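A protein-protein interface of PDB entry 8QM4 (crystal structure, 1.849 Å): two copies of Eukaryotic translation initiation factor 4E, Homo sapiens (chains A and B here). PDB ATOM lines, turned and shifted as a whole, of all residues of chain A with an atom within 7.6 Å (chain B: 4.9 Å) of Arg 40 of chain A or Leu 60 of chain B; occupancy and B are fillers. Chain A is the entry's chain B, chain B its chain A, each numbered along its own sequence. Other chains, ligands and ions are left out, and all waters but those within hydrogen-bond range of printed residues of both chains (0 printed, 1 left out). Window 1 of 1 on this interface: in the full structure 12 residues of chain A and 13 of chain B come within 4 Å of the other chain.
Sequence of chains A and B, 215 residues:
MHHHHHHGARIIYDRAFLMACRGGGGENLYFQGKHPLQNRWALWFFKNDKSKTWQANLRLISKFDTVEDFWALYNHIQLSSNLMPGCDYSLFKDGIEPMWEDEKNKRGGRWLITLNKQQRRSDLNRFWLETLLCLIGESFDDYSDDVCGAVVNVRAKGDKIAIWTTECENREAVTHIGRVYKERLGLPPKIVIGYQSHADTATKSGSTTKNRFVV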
ATOM      1  N   LEU A  37      19.971  18.932   4.617  1.00  0.00           N
ATOM      2  CA  LEU A  37      21.079  18.138   5.156  1.00  0.00           C
ATOM      3  C   LEU A  37      21.529  17.108   4.158  1.00  0.00           C
ATOM      4  O   LEU A  37      20.726  16.695   3.332  1.00  0.00           O
ATOM      5  CB  LEU A  37      20.635  17.456   6.465  1.00  0.00           C
ATOM      6  CG  LEU A  37      20.238  18.366   7.639  1.00  0.00           C
ATOM      7  CD1 LEU A  37      19.797  17.541   8.857  1.00  0.00           C
ATOM      8  CD2 LEU A  37      21.320  19.331   7.970  1.00  0.00           C
ATOM      9  N   GLN A  38      22.803  16.676   4.254  1.00  0.00           N
ATOM     10  CA  GLN A  38      23.379  15.592   3.465  1.00  0.00           C
ATOM     11  C   GLN A  38      22.596  14.312   3.673  1.00  0.00           C
ATOM     12  O   GLN A  38      22.309  13.593   2.714  1.00  0.00           O
ATOM     13  CB  GLN A  38      24.848  15.375   3.892  1.00  0.00           C
ATOM     14  CG  GLN A  38      25.597  14.236   3.202  1.00  0.00           C
ATOM     15  CD  GLN A  38      25.754  14.454   1.706  1.00  0.00           C
ATOM     16  OE1 GLN A  38      25.693  15.578   1.201  1.00  0.00           O
ATOM     17  NE2 GLN A  38      25.979  13.352   0.981  1.00  0.00           N
ATOM     18  N   ASN A  39      22.225  14.034   4.940  1.00  0.00           N
ATOM     19  CA  ASN A  39      21.531  12.833   5.340  1.00  0.00           C
ATOM     20  C   ASN A  39      20.218  13.174   6.000  1.00  0.00           C
ATOM     21  O   ASN A  39      20.054  14.263   6.558  1.00  0.00           O
ATOM     22  CB  ASN A  39      22.421  12.037   6.316  1.00  0.00           C
ATOM     23  CG  ASN A  39      23.548  11.343   5.615  1.00  0.00           C
ATOM     24  OD1 ASN A  39      23.326  10.367   4.897  1.00  0.00           O
ATOM     25  ND2 ASN A  39      24.770  11.812   5.780  1.00  0.00           N
ATOM     26  N   ARG A  40      19.274  12.241   5.957  1.00  0.00           N
ATOM     27  CA  ARG A  40      18.089  12.281   6.794  1.00  0.00           C
ATOM     28  C   ARG A  40      18.470  11.542   8.093  1.00  0.00           C
ATOM     29  O   ARG A  40      19.213  10.570   8.089  1.00  0.00           O
ATOM     30  CB  ARG A  40      16.916  11.604   6.130  1.00  0.00           C
ATOM     31  CG  ARG A  40      15.658  11.640   6.914  1.00  0.00           C
ATOM     32  CD  ARG A  40      14.495  11.586   5.916  1.00  0.00           C
ATOM     33  NE  ARG A  40      13.144  11.752   6.488  1.00  0.00           N
ATOM     34  CZ  ARG A  40      12.242  10.784   6.743  1.00  0.00           C
ATOM     35  NH1 ARG A  40      12.529   9.517   6.501  1.00  0.00           N
ATOM     36  NH2 ARG A  40      11.038  11.096   7.223  1.00  0.00           N
ATOM     37  N   TRP A  41      17.992  12.066   9.208  1.00  0.00           N
ATOM     38  CA  TRP A  41      18.338  11.628  10.555  1.00  0.00           C
ATOM     39  C   TRP A  41      17.058  11.280  11.310  1.00  0.00           C
ATOM     40  O   TRP A  41      16.032  11.873  11.053  1.00  0.00           O
ATOM     41  CB  TRP A  41      19.113  12.747  11.317  1.00  0.00           C
ATOM     42  CG  TRP A  41      20.449  13.056  10.723  1.00  0.00           C
ATOM     43  CD1 TRP A  41      20.711  13.980   9.772  1.00  0.00           C
ATOM     44  CD2 TRP A  41      21.704  12.415  11.015  1.00  0.00           C
ATOM     45  NE1 TRP A  41      22.041  13.960   9.445  1.00  0.00           N
ATOM     46  CE2 TRP A  41      22.670  12.995  10.170  1.00  0.00           C
ATOM     47  CE3 TRP A  41      22.106  11.405  11.902  1.00  0.00           C
ATOM     48  CZ2 TRP A  41      24.021  12.612  10.202  1.00  0.00           C
ATOM     49  CZ3 TRP A  41      23.436  11.030  11.939  1.00  0.00           C
ATOM     50  CH2 TRP A  41      24.379  11.620  11.091  1.00  0.00           C
ATOM     51  N   ALA A  42      17.135  10.319  12.224  1.00  0.00           N
ATOM     52  CA  ALA A  42      16.019   9.881  13.041  1.00  0.00           C
ATOM     53  C   ALA A  42      16.416  10.009  14.479  1.00  0.00           C
ATOM     54  O   ALA A  42      17.506   9.513  14.866  1.00  0.00           O
ATOM     55  CB  ALA A  42      15.674   8.439  12.725  1.00  0.00           C
ATOM     56  N   LEU A  60      10.718   5.689  18.002  1.00  0.00           N
ATOM     57  CA  LEU A  60      11.131   6.707  17.054  1.00  0.00           C
ATOM     58  C   LEU A  60      10.343   7.971  17.347  1.00  0.00           C
ATOM     59  O   LEU A  60       9.114   7.960  17.234  1.00  0.00           O
ATOM     60  CB  LEU A  60      10.863   6.255  15.608  1.00  0.00           C
ATOM     61  CG  LEU A  60      11.032   7.353  14.546  1.00  0.00           C
ATOM     62  CD1 LEU A  60      12.441   7.653  14.349  1.00  0.00           C
ATOM     63  CD2 LEU A  60      10.395   6.947  13.249  1.00  0.00           C
ATOM     64  N   SER A  62      11.076  11.195  15.753  1.00  0.00           N
ATOM     65  CA  SER A  62      10.930  12.056  14.589  1.00  0.00           C
ATOM     66  C   SER A  62      12.093  11.890  13.630  1.00  0.00           C
ATOM     67  O   SER A  62      13.164  11.385  13.994  1.00  0.00           O
ATOM     68  CB  SER A  62      10.784  13.506  15.038  1.00  0.00           C
ATOM     69  OG  SER A  62      10.479  14.347  13.935  1.00  0.00           O
ATOM     70  N   LYS A  63      11.882  12.311  12.410  1.00  0.00           N
ATOM     71  CA  LYS A  63      12.899  12.304  11.354  1.00  0.00           C
ATOM     72  C   LYS A  63      12.961  13.679  10.743  1.00  0.00           C
ATOM     73  O   LYS A  63      11.946  14.392  10.711  1.00  0.00           O
ATOM     74  CB  LYS A  63      12.653  11.225  10.280  1.00  0.00           C
ATOM     75  CG  LYS A  63      12.568   9.826  10.833  1.00  0.00           C
ATOM     76  CD  LYS A  63      12.541   8.791   9.749  1.00  0.00           C
ATOM     77  CE  LYS A  63      12.554   7.351  10.199  1.00  0.00           C
ATOM     78  NZ  LYS A  63      12.596   6.387   9.022  1.00  0.00           N
ATOM     79  N   PHE A  64      14.128  14.052  10.235  1.00  0.00           N
ATOM     80  CA  PHE A  64      14.328  15.348   9.626  1.00  0.00           C
ATOM     81  C   PHE A  64      15.480  15.298   8.675  1.00  0.00           C
ATOM     82  O   PHE A  64      16.365  14.429   8.778  1.00  0.00           O
ATOM     83  CB  PHE A  64      14.488  16.489  10.667  1.00  0.00           C
ATOM     84  CG  PHE A  64      15.716  16.280  11.546  1.00  0.00           C
ATOM     85  CD1 PHE A  64      16.957  16.743  11.153  1.00  0.00           C
ATOM     86  CD2 PHE A  64      15.638  15.523  12.697  1.00  0.00           C
ATOM     87  CE1 PHE A  64      18.101  16.459  11.932  1.00  0.00           C
ATOM     88  CE2 PHE A  64      16.761  15.287  13.476  1.00  0.00           C
ATOM     89  CZ  PHE A  64      17.972  15.769  13.086  1.00  0.00           C
ATOM     90  N   ASP A  65      15.481  16.226   7.727  1.00  0.00           N
ATOM     91  CA  ASP A  65      16.538  16.337   6.745  1.00  0.00           C
ATOM     92  C   ASP A  65      16.841  17.762   6.314  1.00  0.00           C
ATOM     93  O   ASP A  65      17.390  17.961   5.230  1.00  0.00           O
ATOM     94  CB  ASP A  65      16.219  15.439   5.543  1.00  0.00           C
ATOM     95  CG  ASP A  65      14.880  15.779   4.883  1.00  0.00           C
ATOM     96  OD1 ASP A  65      14.351  16.844   5.142  1.00  0.00           O
ATOM     97  OD2 ASP A  65      14.379  14.961   4.135  1.00  0.00           O
ATOM     98  N   THR A  66      16.514  18.742   7.142  1.00  0.00           N
ATOM     99  CA  THR A  66      16.938  20.119   6.972  1.00  0.00           C
ATOM    100  C   THR A  66      17.371  20.684   8.319  1.00  0.00           C
ATOM    101  O   THR A  66      16.947  20.205   9.357  1.00  0.00           O
ATOM    102  CB  THR A  66      15.815  21.024   6.377  1.00  0.00           C
ATOM    103  OG1 THR A  66      14.840  21.303   7.351  1.00  0.00           O
ATOM    104  CG2 THR A  66      15.194  20.482   5.129  1.00  0.00           C
ATOM    105  N   LEU A  91      20.524   9.803  17.949  1.00  0.00           N
ATOM    106  CA  LEU A  91      20.279  10.351  16.613  1.00  0.00           C
ATOM    107  C   LEU A  91      21.063   9.498  15.618  1.00  0.00           C
ATOM    108  O   LEU A  91      22.297   9.491  15.684  1.00  0.00           O
ATOM    109  CB  LEU A  91      20.719  11.824  16.506  1.00  0.00           C
ATOM    110  CG  LEU A  91      20.314  12.488  15.164  1.00  0.00           C
ATOM    111  CD1 LEU A  91      18.852  12.843  15.169  1.00  0.00           C
ATOM    112  CD2 LEU A  91      21.123  13.688  14.827  1.00  0.00           C
ATOM    113  N   PHE A  92      20.377   8.813  14.700  1.00  0.00           N
ATOM    114  CA  PHE A  92      21.008   7.928  13.738  1.00  0.00           C
ATOM    115  C   PHE A  92      20.568   8.256  12.346  1.00  0.00           C
ATOM    116  O   PHE A  92      19.481   8.761  12.106  1.00  0.00           O
ATOM    117  CB  PHE A  92      20.675   6.454  14.069  1.00  0.00           C
ATOM    118  CG  PHE A  92      21.657   5.882  15.081  1.00  0.00           C
ATOM    119  CD1 PHE A  92      21.634   6.290  16.391  1.00  0.00           C
ATOM    120  CD2 PHE A  92      22.611   4.965  14.699  1.00  0.00           C
ATOM    121  CE1 PHE A  92      22.566   5.795  17.312  1.00  0.00           C
ATOM    122  CE2 PHE A  92      23.543   4.498  15.602  1.00  0.00           C
ATOM    123  CZ  PHE A  92      23.486   4.878  16.915  1.00  0.00           C
ATOM    124  N   LYS A  93      21.445   7.966  11.382  1.00  0.00           N
ATOM    125  CA  LYS A  93      21.088   8.122   9.975  1.00  0.00           C
ATOM    126  C   LYS A  93      19.864   7.264   9.677  1.00  0.00           C
ATOM    127  O   LYS A  93      19.704   6.174  10.213  1.00  0.00           O
ATOM    128  CB  LYS A  93      22.251   7.736   9.091  1.00  0.00           C
ATOM    129  CG  LYS A  93      23.397   8.731   9.110  1.00  0.00           C
ATOM    130  CD  LYS A  93      24.568   8.280   8.354  1.00  0.00           C
ATOM    131  CE  LYS A  93      25.600   9.363   8.321  1.00  0.00           C
ATOM    132  NZ  LYS A  93      26.830   8.900   7.673  1.00  0.00           N
ATOM    133  N   ASP A  94      18.985   7.770   8.839  1.00  0.00           N
ATOM    134  CA  ASP A  94      17.759   7.062   8.461  1.00  0.00           C
ATOM    135  C   ASP A  94      18.122   5.656   7.921  1.00  0.00           C
ATOM    136  O   ASP A  94      19.040   5.540   7.090  1.00  0.00           O
ATOM    137  CB  ASP A  94      17.024   7.925   7.425  1.00  0.00           C
ATOM    138  CG  ASP A  94      15.590   7.563   7.144  1.00  0.00           C
ATOM    139  OD1 ASP A  94      14.999   6.789   7.942  1.00  0.00           O
ATOM    140  OD2 ASP A  94      15.047   8.083   6.152  1.00  0.00           O
ATOM    141  N   GLY A  95      17.469   4.635   8.447  1.00  0.00           N
ATOM    142  CA  GLY A  95      17.713   3.269   8.051  1.00  0.00           C
ATOM    143  C   GLY A  95      18.697   2.504   8.921  1.00  0.00           C
ATOM    144  O   GLY A  95      18.975   1.335   8.636  1.00  0.00           O
ATOM    145  N   ILE A 136      24.974  16.348  11.936  1.00  0.00           N
ATOM    146  CA  ILE A 136      24.110  16.882  10.882  1.00  0.00           C
ATOM    147  C   ILE A 136      24.915  17.759   9.896  1.00  0.00           C
ATOM    148  O   ILE A 136      24.537  17.805   8.739  1.00  0.00           O
ATOM    149  CB  ILE A 136      22.854  17.586  11.404  1.00  0.00           C
ATOM    150  CG1 ILE A 136      23.210  18.924  12.096  1.00  0.00           C
ATOM    151  CG2 ILE A 136      22.047  16.648  12.355  1.00  0.00           C
ATOM    152  CD1 ILE A 136      22.056  19.738  12.526  1.00  0.00           C
ATOM    153  N   GLU A 138      27.999  17.194   8.856  1.00  0.00           N
ATOM    154  CA  GLU A 138      28.980  16.373   8.160  1.00  0.00           C
ATOM    155  C   GLU A 138      30.408  16.875   8.380  1.00  0.00           C
ATOM    156  O   GLU A 138      31.133  17.120   7.428  1.00  0.00           O
ATOM    157  CB  GLU A 138      28.640  16.272   6.666  1.00  0.00           C
ATOM    158  CG  GLU A 138      27.251  15.731   6.359  1.00  0.00           C
ATOM    159  CD  GLU A 138      27.066  14.237   6.586  1.00  0.00           C
ATOM    160  OE1 GLU A 138      27.960  13.466   6.176  1.00  0.00           O
ATOM    161  OE2 GLU A 138      26.023  13.823   7.144  1.00  0.00           O
ATOM    162  N   CYS A 148      27.487   6.507  12.057  1.00  0.00           N
ATOM    163  CA  CYS A 148      26.142   5.945  12.117  1.00  0.00           C
ATOM    164  C   CYS A 148      25.184   6.868  12.903  1.00  0.00           C
ATOM    165  O   CYS A 148      24.061   7.104  12.487  1.00  0.00           O
ATOM    166  CB  CYS A 148      26.195   4.565  12.747  1.00  0.00           C
ATOM    167  SG  CYS A 148      27.162   3.401  11.751  1.00  0.00           S
ATOM    168  N   ALA B  42      15.451  13.988  -4.269  1.00  0.00           N
ATOM    169  CA  ALA B  42      15.603  12.982  -3.262  1.00  0.00           C
ATOM    170  C   ALA B  42      14.682  11.831  -3.600  1.00  0.00           C
ATOM    171  O   ALA B  42      13.469  12.072  -3.875  1.00  0.00           O
ATOM    172  CB  ALA B  42      15.244  13.540  -1.896  1.00  0.00           C
ATOM    173  N   LEU B  43      15.205  10.615  -3.584  1.00  0.00           N
ATOM    174  CA  LEU B  43      14.427   9.392  -3.771  1.00  0.00           C
ATOM    175  C   LEU B  43      14.084   8.823  -2.421  1.00  0.00           C
ATOM    176  O   LEU B  43      14.978   8.609  -1.612  1.00  0.00           O
ATOM    177  CB  LEU B  43      15.197   8.326  -4.554  1.00  0.00           C
ATOM    178  CG  LEU B  43      14.466   6.995  -4.744  1.00  0.00           C
ATOM    179  CD1 LEU B  43      13.242   7.173  -5.594  1.00  0.00           C
ATOM    180  CD2 LEU B  43      15.361   5.995  -5.329  1.00  0.00           C
ATOM    181  N   TRP B  44      12.820   8.554  -2.209  1.00  0.00           N
ATOM    182  CA  TRP B  44      12.252   8.007  -0.996  1.00  0.00           C
ATOM    183  C   TRP B  44      11.606   6.687  -1.237  1.00  0.00           C
ATOM    184  O   TRP B  44      11.109   6.379  -2.367  1.00  0.00           O
ATOM    185  CB  TRP B  44      11.157   8.948  -0.457  1.00  0.00           C
ATOM    186  CG  TRP B  44      11.546  10.349  -0.206  1.00  0.00           C
ATOM    187  CD1 TRP B  44      11.716  11.362  -1.103  1.00  0.00           C
ATOM    188  CD2 TRP B  44      11.854  10.897   1.074  1.00  0.00           C
ATOM    189  NE1 TRP B  44      12.099  12.504  -0.456  1.00  0.00           N
ATOM    190  CE2 TRP B  44      12.207  12.247   0.880  1.00  0.00           C
ATOM    191  CE3 TRP B  44      11.875  10.362   2.369  1.00  0.00           C
ATOM    192  CZ2 TRP B  44      12.533  13.092   1.931  1.00  0.00           C
ATOM    193  CZ3 TRP B  44      12.217  11.203   3.405  1.00  0.00           C
ATOM    194  CH2 TRP B  44      12.550  12.546   3.178  1.00  0.00           C
ATOM    195  N   LEU B  58       9.088   5.218   6.252  1.00  0.00           N
ATOM    196  CA  LEU B  58       9.523   6.157   5.224  1.00  0.00           C
ATOM    197  C   LEU B  58      11.000   6.360   5.327  1.00  0.00           C
ATOM    198  O   LEU B  58      11.475   6.815   6.374  1.00  0.00           O
ATOM    199  CB  LEU B  58       8.783   7.507   5.364  1.00  0.00           C
ATOM    200  CG  LEU B  58       9.187   8.590   4.331  1.00  0.00           C
ATOM    201  CD1 LEU B  58       8.864   8.172   2.905  1.00  0.00           C
ATOM    202  CD2 LEU B  58       8.536   9.935   4.685  1.00  0.00           C
ATOM    203  N   ARG B  59      11.743   6.045   4.260  1.00  0.00           N
ATOM    204  CA  ARG B  59      13.197   6.127   4.243  1.00  0.00           C
ATOM    205  C   ARG B  59      13.672   6.967   3.063  1.00  0.00           C
ATOM    206  O   ARG B  59      13.166   6.815   1.938  1.00  0.00           O
ATOM    207  CB  ARG B  59      13.778   4.692   4.121  1.00  0.00           C
ATOM    208  CG  ARG B  59      14.549   4.137   5.336  1.00  0.00           C
ATOM    209  CD  ARG B  59      15.368   2.936   4.868  1.00  0.00           C
ATOM    210  NE  ARG B  59      16.831   3.007   4.601  1.00  0.00           N
ATOM    211  CZ  ARG B  59      17.602   4.039   4.233  1.00  0.00           C
ATOM    212  NH1 ARG B  59      18.900   3.865   4.034  1.00  0.00           N
ATOM    213  NH2 ARG B  59      17.089   5.251   4.075  1.00  0.00           N
ATOM    214  N   LEU B  60      14.613   7.868   3.297  1.00  0.00           N
ATOM    215  CA  LEU B  60      15.332   8.552   2.240  1.00  0.00           C
ATOM    216  C   LEU B  60      16.409   7.635   1.707  1.00  0.00           C
ATOM    217  O   LEU B  60      17.293   7.264   2.468  1.00  0.00           O
ATOM    218  CB  LEU B  60      15.972   9.839   2.753  1.00  0.00           C
ATOM    219  CG  LEU B  60      16.985  10.506   1.770  1.00  0.00           C
ATOM    220  CD1 LEU B  60      16.267  11.129   0.679  1.00  0.00           C
ATOM    221  CD2 LEU B  60      17.863  11.487   2.474  1.00  0.00           C
ATOM    222  N   ILE B  61      16.371   7.271   0.425  1.00  0.00           N
ATOM    223  CA  ILE B  61      17.378   6.407  -0.195  1.00  0.00           C
ATOM    224  C   ILE B  61      18.614   7.224  -0.583  1.00  0.00           C
ATOM    225  O   ILE B  61      19.741   6.901  -0.165  1.00  0.00           O
ATOM    226  CB  ILE B  61      16.799   5.636  -1.407  1.00  0.00           C
ATOM    227  CG1 ILE B  61      15.597   4.824  -0.994  1.00  0.00           C
ATOM    228  CG2 ILE B  61      17.874   4.768  -2.079  1.00  0.00           C
ATOM    229  CD1 ILE B  61      15.781   3.983   0.262  1.00  0.00           C
ATOM    230  N   SER B  62      18.413   8.316  -1.314  1.00  0.00           N
ATOM    231  CA  SER B  62      19.521   9.011  -1.938  1.00  0.00           C
ATOM    232  C   SER B  62      19.104  10.325  -2.513  1.00  0.00           C
ATOM    233  O   SER B  62      17.917  10.586  -2.762  1.00  0.00           O
ATOM    234  CB  SER B  62      20.151   8.101  -3.020  1.00  0.00           C
ATOM    235  OG  SER B  62      21.348   8.679  -3.535  1.00  0.00           O
ATOM    236  N   LYS B  63      20.075  11.186  -2.737  1.00  0.00           N
ATOM    237  CA  LYS B  63      19.874  12.501  -3.348  1.00  0.00           C
ATOM    238  C   LYS B  63      20.835  12.622  -4.515  1.00  0.00           C
ATOM    239  O   LYS B  63      21.904  11.976  -4.506  1.00  0.00           O
ATOM    240  CB  LYS B  63      20.027  13.659  -2.354  1.00  0.00           C
ATOM    241  CG  LYS B  63      19.080  13.560  -1.159  1.00  0.00           C
ATOM    242  CD  LYS B  63      19.126  14.798  -0.325  1.00  0.00           C
ATOM    243  CE  LYS B  63      18.151  14.834   0.830  1.00  0.00           C
ATOM    244  NZ  LYS B  63      18.214  16.159   1.572  1.00  0.00           N
ATOM    245  N   GLU B  97       9.126  16.792   1.829  1.00  0.00           N
ATOM    246  CA  GLU B  97       8.719  15.450   2.189  1.00  0.00           C
ATOM    247  C   GLU B  97       7.590  14.923   1.305  1.00  0.00           C
ATOM    248  O   GLU B  97       6.707  15.696   0.921  1.00  0.00           O
ATOM    249  CB  GLU B  97       8.369  15.362   3.653  1.00  0.00           C
ATOM    250  CG  GLU B  97       9.553  15.750   4.521  1.00  0.00           C
ATOM    251  CD  GLU B  97       9.460  15.368   5.983  1.00  0.00           C
ATOM    252  OE1 GLU B  97       8.330  15.267   6.506  1.00  0.00           O
ATOM    253  OE2 GLU B  97      10.532  15.162   6.604  1.00  0.00           O
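Positions printed for both chains: 42, 60, 62 and 63. Of the 10 pairs that touch across the chains among the printed residues, none has its exchanged pair printed and touching as well.
Printed residues of chain B that touch a printed residue of chain A: Trp 44, Leu 58, Arg 59, Leu 60 and Lys 63. Hydrophobic or aromatic side chains of chain B that line the printed part of chain A: Trp 44, Leu 58 and Leu 60. Printed residues of chain A that touch a printed residue of chain B: Leu 37, Arg 40, Lys 63, Asp 65, Asp 94 and Gly 95.
Of chain B, only Trp 44 (3.3 Å), Leu 58 (2.9 Å) and Leu 60 (3.8 Å) come within 4 Å of Arg 40 of chain A. Of the printed residues of chain A, Leu 60 of chain B touches Arg 40 (3.8 Å) and Asp 94 (2.9 Å). Of the printed residues of chain A, Arg 59 of chain B touches Asp 94 and Gly 95. Of the printed residues of chain B, Leu 37 of chain A touches Lys 63 (3.1 Å). Printed residues of chain B within 4 Å of Asp 65 of chain A: Trp 44 (3.2 Å). Printed residues of chain B within 4 Å of Gly 95 of chain A: Arg 59 (3.6 Å).
The side-chain amino group of Lys 63 of chain A sits at hydrogen-bond distance from the backbone carbonyl oxygen of Leu 58 of chain B (2.9 Å). The backbone carbonyl oxygen (O) of Leu 37 of chain A is in hydrogen-bond range of the side-chain amino group (NZ) of Lys 63 of chain B, 3.1 Å away. NH1 of Arg 40 of chain A is in hydrogen-bond range of O of Leu 58 of chain B (2.9 Å). The guanidinium group of Arg 59 of chain B is in hydrogen-bond range of the backbone carbonyl oxygen of Asp 94 of chain A, at 3.5 Å. N of Leu 60 of chain B lies within hydrogen-bond range of OD2 of Asp 94 of chain A.
Among the printed residues, pairs that only touch across the chains: Arg 40 of chain A with Trp 44 of chain B (3.3 Å), Arg 40 of chain A with Leu 60 of chain B (3.8 Å), Asp 65 of chain A with Trp 44 of chain B (3.2 Å), Asp 94 of chain A with Leu 58 of chain B (3.8 Å) and Gly 95 of chain A with Arg 59 of chain B (3.6 Å).
N of Leu 37 of chain A is in hydrogen-bond range of O of Asp 65 of chain A (2.8 Å). The guanidinium group of Arg 40 of chain A is in salt-bridge range of the side-chain carboxylate of Asp 94 of chain A (2.9 Å). The side-chain amino group (NZ) of Lys 63 of chain A is in salt-bridge range of the side-chain carboxylate (OD1) of Asp 94 of chain A (2.7 Å).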
